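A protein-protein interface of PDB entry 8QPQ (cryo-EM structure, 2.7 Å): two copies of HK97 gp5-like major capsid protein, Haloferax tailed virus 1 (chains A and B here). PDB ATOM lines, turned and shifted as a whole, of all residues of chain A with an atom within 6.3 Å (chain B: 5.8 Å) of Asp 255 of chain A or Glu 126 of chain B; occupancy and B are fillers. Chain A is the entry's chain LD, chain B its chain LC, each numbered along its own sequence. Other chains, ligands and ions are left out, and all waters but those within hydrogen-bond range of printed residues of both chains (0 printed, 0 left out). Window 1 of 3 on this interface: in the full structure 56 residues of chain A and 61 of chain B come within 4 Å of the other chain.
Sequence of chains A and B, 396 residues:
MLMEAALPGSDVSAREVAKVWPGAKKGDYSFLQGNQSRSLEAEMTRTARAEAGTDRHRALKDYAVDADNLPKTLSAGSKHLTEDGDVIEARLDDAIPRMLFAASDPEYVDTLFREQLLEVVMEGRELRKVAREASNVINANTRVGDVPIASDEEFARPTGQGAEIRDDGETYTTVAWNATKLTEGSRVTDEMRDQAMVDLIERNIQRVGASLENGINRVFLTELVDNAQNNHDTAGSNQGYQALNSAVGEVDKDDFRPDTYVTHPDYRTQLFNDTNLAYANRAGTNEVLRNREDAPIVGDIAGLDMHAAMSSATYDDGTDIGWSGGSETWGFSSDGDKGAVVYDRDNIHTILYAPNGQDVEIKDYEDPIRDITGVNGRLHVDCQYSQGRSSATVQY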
ATOM      1  N   ASP A 152      -5.938 -26.607  -9.791  1.00  0.00           N
ATOM      2  CA  ASP A 152      -6.863 -25.560  -9.375  1.00  0.00           C
ATOM      3  C   ASP A 152      -7.158 -24.586 -10.520  1.00  0.00           C
ATOM      4  O   ASP A 152      -6.302 -24.313 -11.379  1.00  0.00           O
ATOM      5  CB  ASP A 152      -6.308 -24.740  -8.220  1.00  0.00           C
ATOM      6  CG  ASP A 152      -6.095 -25.487  -6.916  1.00  0.00           C
ATOM      7  OD1 ASP A 152      -6.566 -26.638  -6.778  1.00  0.00           O
ATOM      8  OD2 ASP A 152      -5.453 -24.898  -6.028  1.00  0.00           O
ATOM      9  N   GLU A 153      -8.373 -24.021 -10.473  1.00  0.00           N
ATOM     10  CA  GLU A 153      -8.753 -22.957 -11.386  1.00  0.00           C
ATOM     11  C   GLU A 153      -7.905 -21.718 -11.133  1.00  0.00           C
ATOM     12  O   GLU A 153      -7.701 -21.333  -9.999  1.00  0.00           O
ATOM     13  CB  GLU A 153     -10.241 -22.683 -11.312  1.00  0.00           C
ATOM     14  CG  GLU A 153     -10.768 -22.132 -10.005  1.00  0.00           C
ATOM     15  CD  GLU A 153     -12.288 -22.041 -10.001  1.00  0.00           C
ATOM     16  OE1 GLU A 153     -12.935 -22.965 -10.545  1.00  0.00           O
ATOM     17  OE2 GLU A 153     -12.845 -21.048  -9.442  1.00  0.00           O
ATOM     18  N   GLU A 250     -10.151 -22.483   8.008  1.00  0.00           N
ATOM     19  CA  GLU A 250      -8.950 -22.922   7.308  1.00  0.00           C
ATOM     20  C   GLU A 250      -9.276 -23.605   5.978  1.00  0.00           C
ATOM     21  O   GLU A 250      -8.634 -23.332   4.969  1.00  0.00           O
ATOM     22  CB  GLU A 250      -8.114 -23.831   8.208  1.00  0.00           C
ATOM     23  CG  GLU A 250      -7.494 -23.101   9.401  1.00  0.00           C
ATOM     24  CD  GLU A 250      -6.441 -22.091   8.968  1.00  0.00           C
ATOM     25  OE1 GLU A 250      -5.416 -22.554   8.428  1.00  0.00           O
ATOM     26  OE2 GLU A 250      -6.597 -20.853   9.198  1.00  0.00           O
ATOM     27  N   VAL A 251     -10.282 -24.482   5.966  1.00  0.00           N
ATOM     28  CA  VAL A 251     -10.716 -25.178   4.761  1.00  0.00           C
ATOM     29  C   VAL A 251     -11.352 -24.197   3.765  1.00  0.00           C
ATOM     30  O   VAL A 251     -11.100 -24.289   2.564  1.00  0.00           O
ATOM     31  CB  VAL A 251     -11.637 -26.369   5.109  1.00  0.00           C
ATOM     32  CG1 VAL A 251     -12.055 -27.124   3.870  1.00  0.00           C
ATOM     33  CG2 VAL A 251     -10.934 -27.342   6.039  1.00  0.00           C
ATOM     34  N   ASP A 252     -12.141 -23.236   4.265  1.00  0.00           N
ATOM     35  CA  ASP A 252     -12.757 -22.156   3.508  1.00  0.00           C
ATOM     36  C   ASP A 252     -11.697 -21.270   2.841  1.00  0.00           C
ATOM     37  O   ASP A 252     -11.853 -20.832   1.705  1.00  0.00           O
ATOM     38  CB  ASP A 252     -13.690 -21.384   4.449  1.00  0.00           C
ATOM     39  CG  ASP A 252     -14.565 -20.316   3.799  1.00  0.00           C
ATOM     40  OD1 ASP A 252     -14.829 -20.422   2.584  1.00  0.00           O
ATOM     41  OD2 ASP A 252     -14.983 -19.375   4.518  1.00  0.00           O
ATOM     42  N   LYS A 253     -10.584 -21.008   3.549  1.00  0.00           N
ATOM     43  CA  LYS A 253      -9.461 -20.219   3.048  1.00  0.00           C
ATOM     44  C   LYS A 253      -8.715 -20.915   1.908  1.00  0.00           C
ATOM     45  O   LYS A 253      -8.184 -20.241   1.042  1.00  0.00           O
ATOM     46  CB  LYS A 253      -8.555 -19.886   4.228  1.00  0.00           C
ATOM     47  CG  LYS A 253      -7.332 -19.036   3.979  1.00  0.00           C
ATOM     48  CD  LYS A 253      -6.877 -18.337   5.241  1.00  0.00           C
ATOM     49  CE  LYS A 253      -6.303 -19.250   6.311  1.00  0.00           C
ATOM     50  NZ  LYS A 253      -6.097 -18.522   7.580  1.00  0.00           N
ATOM     51  N   ASP A 254      -8.698 -22.250   1.892  1.00  0.00           N
ATOM     52  CA  ASP A 254      -8.208 -23.029   0.764  1.00  0.00           C
ATOM     53  C   ASP A 254      -9.311 -23.338  -0.265  1.00  0.00           C
ATOM     54  O   ASP A 254      -9.122 -24.161  -1.139  1.00  0.00           O
ATOM     55  CB  ASP A 254      -7.494 -24.299   1.242  1.00  0.00           C
ATOM     56  CG  ASP A 254      -6.218 -24.136   2.053  1.00  0.00           C
ATOM     57  OD1 ASP A 254      -5.813 -23.031   2.433  1.00  0.00           O
ATOM     58  OD2 ASP A 254      -5.605 -25.162   2.355  1.00  0.00           O
ATOM     59  N   ASP A 255     -10.468 -22.669  -0.176  1.00  0.00           N
ATOM     60  CA  ASP A 255     -11.596 -22.681  -1.106  1.00  0.00           C
ATOM     61  C   ASP A 255     -12.260 -24.056  -1.271  1.00  0.00           C
ATOM     62  O   ASP A 255     -12.724 -24.410  -2.360  1.00  0.00           O
ATOM     63  CB  ASP A 255     -11.253 -22.003  -2.435  1.00  0.00           C
ATOM     64  CG  ASP A 255     -10.609 -20.646  -2.272  1.00  0.00           C
ATOM     65  OD1 ASP A 255     -11.262 -19.749  -1.727  1.00  0.00           O
ATOM     66  OD2 ASP A 255      -9.478 -20.491  -2.781  1.00  0.00           O
ATOM     67  N   PHE A 256     -12.374 -24.795  -0.162  1.00  0.00           N
ATOM     68  CA  PHE A 256     -13.179 -26.007  -0.076  1.00  0.00           C
ATOM     69  C   PHE A 256     -14.271 -25.834   0.981  1.00  0.00           C
ATOM     70  O   PHE A 256     -14.139 -25.012   1.884  1.00  0.00           O
ATOM     71  CB  PHE A 256     -12.297 -27.225   0.219  1.00  0.00           C
ATOM     72  CG  PHE A 256     -11.346 -27.594  -0.892  1.00  0.00           C
ATOM     73  CD1 PHE A 256     -11.788 -28.331  -1.985  1.00  0.00           C
ATOM     74  CD2 PHE A 256     -10.018 -27.184  -0.868  1.00  0.00           C
ATOM     75  CE1 PHE A 256     -10.925 -28.649  -3.025  1.00  0.00           C
ATOM     76  CE2 PHE A 256      -9.162 -27.487  -1.918  1.00  0.00           C
ATOM     77  CZ  PHE A 256      -9.617 -28.218  -2.993  1.00  0.00           C
ATOM     78  N   ARG A 257     -15.345 -26.625   0.886  1.00  0.00           N
ATOM     79  CA  ARG A 257     -16.420 -26.578   1.868  1.00  0.00           C
ATOM     80  C   ARG A 257     -16.503 -27.908   2.600  1.00  0.00           C
ATOM     81  O   ARG A 257     -16.909 -28.890   2.002  1.00  0.00           O
ATOM     82  CB  ARG A 257     -17.744 -26.144   1.231  1.00  0.00           C
ATOM     83  CG  ARG A 257     -17.587 -24.772   0.583  1.00  0.00           C
ATOM     84  CD  ARG A 257     -18.886 -24.040   0.278  1.00  0.00           C
ATOM     85  NE  ARG A 257     -19.218 -23.304   1.485  1.00  0.00           N
ATOM     86  CZ  ARG A 257     -20.232 -23.566   2.304  1.00  0.00           C
ATOM     87  NH1 ARG A 257     -20.420 -22.808   3.373  1.00  0.00           N
ATOM     88  NH2 ARG A 257     -21.079 -24.556   2.060  1.00  0.00           N
ATOM     89  N   GLY B 124     -10.026 -29.569  -8.960  1.00  0.00           N
ATOM     90  CA  GLY B 124      -9.245 -28.681  -8.117  1.00  0.00           C
ATOM     91  C   GLY B 124     -10.120 -27.752  -7.281  1.00  0.00           C
ATOM     92  O   GLY B 124     -11.340 -27.845  -7.264  1.00  0.00           O
ATOM     93  N   ARG B 125      -9.458 -26.838  -6.576  1.00  0.00           N
ATOM     94  CA  ARG B 125     -10.060 -25.739  -5.849  1.00  0.00           C
ATOM     95  C   ARG B 125     -10.967 -24.899  -6.756  1.00  0.00           C
ATOM     96  O   ARG B 125     -10.605 -24.613  -7.902  1.00  0.00           O
ATOM     97  CB  ARG B 125      -8.862 -24.894  -5.391  1.00  0.00           C
ATOM     98  CG  ARG B 125      -9.142 -23.749  -4.440  1.00  0.00           C
ATOM     99  CD  ARG B 125      -7.812 -23.202  -3.952  1.00  0.00           C
ATOM    100  NE  ARG B 125      -7.567 -21.835  -4.385  1.00  0.00           N
ATOM    101  CZ  ARG B 125      -6.615 -21.445  -5.223  1.00  0.00           C
ATOM    102  NH1 ARG B 125      -6.505 -20.167  -5.535  1.00  0.00           N
ATOM    103  NH2 ARG B 125      -5.735 -22.299  -5.714  1.00  0.00           N
ATOM    104  N   GLU B 126     -12.174 -24.560  -6.276  1.00  0.00           N
ATOM    105  CA  GLU B 126     -13.066 -23.655  -6.984  1.00  0.00           C
ATOM    106  C   GLU B 126     -13.224 -22.341  -6.215  1.00  0.00           C
ATOM    107  O   GLU B 126     -13.660 -22.341  -5.071  1.00  0.00           O
ATOM    108  CB  GLU B 126     -14.432 -24.313  -7.268  1.00  0.00           C
ATOM    109  CG  GLU B 126     -15.493 -23.307  -7.696  1.00  0.00           C
ATOM    110  CD  GLU B 126     -16.474 -23.755  -8.769  1.00  0.00           C
ATOM    111  OE1 GLU B 126     -16.683 -24.974  -8.859  1.00  0.00           O
ATOM    112  OE2 GLU B 126     -16.953 -22.881  -9.531  1.00  0.00           O
ATOM    113  N   LEU B 127     -12.960 -21.225  -6.887  1.00  0.00           N
ATOM    114  CA  LEU B 127     -13.069 -19.917  -6.244  1.00  0.00           C
ATOM    115  C   LEU B 127     -14.523 -19.443  -6.242  1.00  0.00           C
ATOM    116  O   LEU B 127     -15.314 -19.777  -7.116  1.00  0.00           O
ATOM    117  CB  LEU B 127     -12.162 -18.892  -6.928  1.00  0.00           C
ATOM    118  CG  LEU B 127     -10.715 -19.297  -7.175  1.00  0.00           C
ATOM    119  CD1 LEU B 127      -9.938 -18.106  -7.653  1.00  0.00           C
ATOM    120  CD2 LEU B 127     -10.059 -19.808  -5.909  1.00  0.00           C
ATOM    121  N   ARG B 128     -14.862 -18.624  -5.244  1.00  0.00           N
ATOM    122  CA  ARG B 128     -16.194 -18.058  -5.101  1.00  0.00           C
ATOM    123  C   ARG B 128     -16.433 -16.971  -6.148  1.00  0.00           C
ATOM    124  O   ARG B 128     -15.641 -16.043  -6.281  1.00  0.00           O
ATOM    125  CB  ARG B 128     -16.382 -17.540  -3.668  1.00  0.00           C
ATOM    126  CG  ARG B 128     -16.422 -18.679  -2.671  1.00  0.00           C
ATOM    127  CD  ARG B 128     -16.343 -18.148  -1.263  1.00  0.00           C
ATOM    128  NE  ARG B 128     -16.385 -19.080  -0.175  1.00  0.00           N
ATOM    129  CZ  ARG B 128     -17.462 -19.446   0.508  1.00  0.00           C
ATOM    130  NH1 ARG B 128     -17.339 -20.186   1.585  1.00  0.00           N
ATOM    131  NH2 ARG B 128     -18.675 -19.091   0.098  1.00  0.00           N
ATOM    132  N   LYS B 129     -17.548 -17.103  -6.869  1.00  0.00           N
ATOM    133  CA  LYS B 129     -17.914 -16.211  -7.959  1.00  0.00           C
ATOM    134  C   LYS B 129     -19.170 -15.445  -7.560  1.00  0.00           C
ATOM    135  O   LYS B 129     -20.226 -16.054  -7.410  1.00  0.00           O
ATOM    136  CB  LYS B 129     -18.098 -17.025  -9.240  1.00  0.00           C
ATOM    137  CG  LYS B 129     -16.805 -17.668  -9.728  1.00  0.00           C
ATOM    138  CD  LYS B 129     -17.034 -18.830 -10.674  1.00  0.00           C
ATOM    139  CE  LYS B 129     -15.747 -19.581 -10.949  1.00  0.00           C
ATOM    140  NZ  LYS B 129     -15.438 -20.505  -9.833  1.00  0.00           N
ATOM    141  N   PRO B 265     -12.262 -14.928   3.793  1.00  0.00           N
ATOM    142  CA  PRO B 265     -12.422 -16.088   4.679  1.00  0.00           C
ATOM    143  C   PRO B 265     -12.017 -15.879   6.138  1.00  0.00           C
ATOM    144  O   PRO B 265     -12.703 -16.379   7.031  1.00  0.00           O
ATOM    145  CB  PRO B 265     -11.483 -17.141   4.056  1.00  0.00           C
ATOM    146  CG  PRO B 265     -11.455 -16.802   2.584  1.00  0.00           C
ATOM    147  CD  PRO B 265     -11.569 -15.293   2.555  1.00  0.00           C
ATOM    148  N   MET B 310     -16.269 -14.040  -0.611  1.00  0.00           N
ATOM    149  CA  MET B 310     -15.212 -14.108  -1.613  1.00  0.00           C
ATOM    150  C   MET B 310     -14.032 -14.950  -1.143  1.00  0.00           C
ATOM    151  O   MET B 310     -13.895 -15.237   0.025  1.00  0.00           O
ATOM    152  CB  MET B 310     -14.790 -12.709  -2.081  1.00  0.00           C
ATOM    153  CG  MET B 310     -15.942 -12.109  -2.889  1.00  0.00           C
ATOM    154  SD  MET B 310     -15.530 -10.843  -4.113  1.00  0.00           S
ATOM    155  CE  MET B 310     -14.761 -11.841  -5.394  1.00  0.00           C
ATOM    156  N   SER B 311     -13.202 -15.398  -2.087  1.00  0.00           N
ATOM    157  CA  SER B 311     -12.014 -16.205  -1.858  1.00  0.00           C
ATOM    158  C   SER B 311     -10.798 -15.332  -1.537  1.00  0.00           C
ATOM    159  O   SER B 311     -10.745 -14.157  -1.866  1.00  0.00           O
ATOM    160  CB  SER B 311     -11.739 -17.003  -3.102  1.00  0.00           C
ATOM    161  OG  SER B 311     -12.666 -18.060  -3.213  1.00  0.00           O
ATOM    162  N   SER B 312      -9.773 -15.928  -0.919  1.00  0.00           N
ATOM    163  CA  SER B 312      -8.535 -15.228  -0.577  1.00  0.00           C
ATOM    164  C   SER B 312      -7.742 -14.833  -1.831  1.00  0.00           C
ATOM    165  O   SER B 312      -7.158 -13.752  -1.890  1.00  0.00           O
ATOM    166  CB  SER B 312      -7.716 -16.094   0.351  1.00  0.00           C
ATOM    167  OG  SER B 312      -6.615 -15.359   0.854  1.00  0.00           O
ATOM    168  N   ALA B 313      -7.773 -15.669  -2.868  1.00  0.00           N
ATOM    169  CA  ALA B 313      -6.997 -15.476  -4.087  1.00  0.00           C
ATOM    170  C   ALA B 313      -7.550 -14.389  -5.021  1.00  0.00           C
ATOM    171  O   ALA B 313      -6.805 -13.989  -5.936  1.00  0.00           O
ATOM    172  CB  ALA B 313      -6.885 -16.792  -4.809  1.00  0.00           C
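OD2 of Asp 255 of chain A lies within salt-bridge range of NE of Arg 125 of chain B, at 2.8 Å.
The side-chain carboxylate (OD1) of Asp 255 of chain A is in hydrogen-bond range of the side-chain hydroxyl (OG) of Ser 311 of chain B, at 2.7 Å.
NH1 of Arg 128 of chain B lies within salt-bridge range of OD1 of Asp 252 of chain A.
NH2 of Arg 125 of chain B is in salt-bridge range of OD2 of Asp 152 of chain A.
The backbone carbonyl oxygen (O) of Arg 125 of chain B sits close to the backbone NH (N) of Glu 153 of chain A, at 3.5 Å.
OE2 of Glu 153 of chain A lies within salt-bridge range of NZ of Lys 129 of chain B (2.7 Å).
N of Leu 127 of chain B lies within hydrogen-bond range of OE2 of Glu 153 of chain A.
N of Arg 128 of chain B is in hydrogen-bond range of OG of Ser 311 of chain B (3.0 Å).
OE2 of Glu 126 of chain B lies within salt-bridge range of NZ of Lys 129 of chain B, 2.8 Å away.
The side-chain carboxylate (OE2) of Glu 250 of chain A is in salt-bridge range of the side-chain amino group (NZ) of Lys 253 of chain A (2.9 Å).
The backbone carbonyl oxygen (O) of Leu 127 of chain B sits at hydrogen-bond distance from the side-chain amino group (NZ) of Lys 129 of chain B, at 2.8 Å.
N of Phe 256 of chain A sits at hydrogen-bond distance from O of Val 251 of chain A (3.1 Å).
Gly 124 of chain B touches Asp 152 of chain A.
Glu 153 of chain A touches Glu 126 of chain B (OE2 to C, 3.5 Å).
Lys 253 of chain A touches Pro 265 of chain B.
O of Asp 254 of chain A touches CD of Arg 125 of chain B, at 3.2 Å.
Asp 255 of chain A touches Glu 126 of chain B (O to O, 3.5 Å).
Leu 127 of chain B touches Asp 255 of chain A (CD2 to OD2, 3.3 Å).
Arg 125 of chain B touches Phe 256 of chain A.
NE of Arg 257 of chain A touches NH1 of Arg 128 of chain B, at 3.6 Å.
Asp 255 of chain A touches four residues of chain B.
Glu 126 of chain B touches just these residues of chain A: Glu 153 and Asp 255.
Of the printed residues of chain B, Asp 152 of chain A touches Gly 124 and Arg 125.
Of the printed residues of chain A, Lys 129 of chain B touches Glu 153 (2.7 Å).
Printed residues of chain B within 4 Å of Lys 253 of chain A: Pro 265 (3.8 Å).
Printed residues of chain A within 4 Å of Arg 128 of chain B: Asp 252 (2.7 Å) and Arg 257 (3.6 Å).
Met 310 of chain B touches none of the printed residues of chain A.
Of the 10 printed residues of chain A, 8 touch a printed residue of chain B.
Along chain B the printed residues that touch a printed residue of chain A span positions 124 to 311.
Among the printed residues, 15 pairs touch across the chains.
Among the printed residues, Asp or Glu carboxylates within 4 Å of a Lys or Arg side-chain nitrogen of the other chain: Asp 152 of chain A with Arg 125 of chain B (2.6 Å), Glu 153 of chain A with Lys 129 of chain B (2.7 Å), Asp 252 of chain A with Arg 128 of chain B (2.7 Å) and Asp 255 of chain A with Arg 125 of chain B (2.8 Å).
No position is printed for both chains.
Of the 15 pairs that touch across the chains among the printed residues, none has its exchanged pair printed and touching as well.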
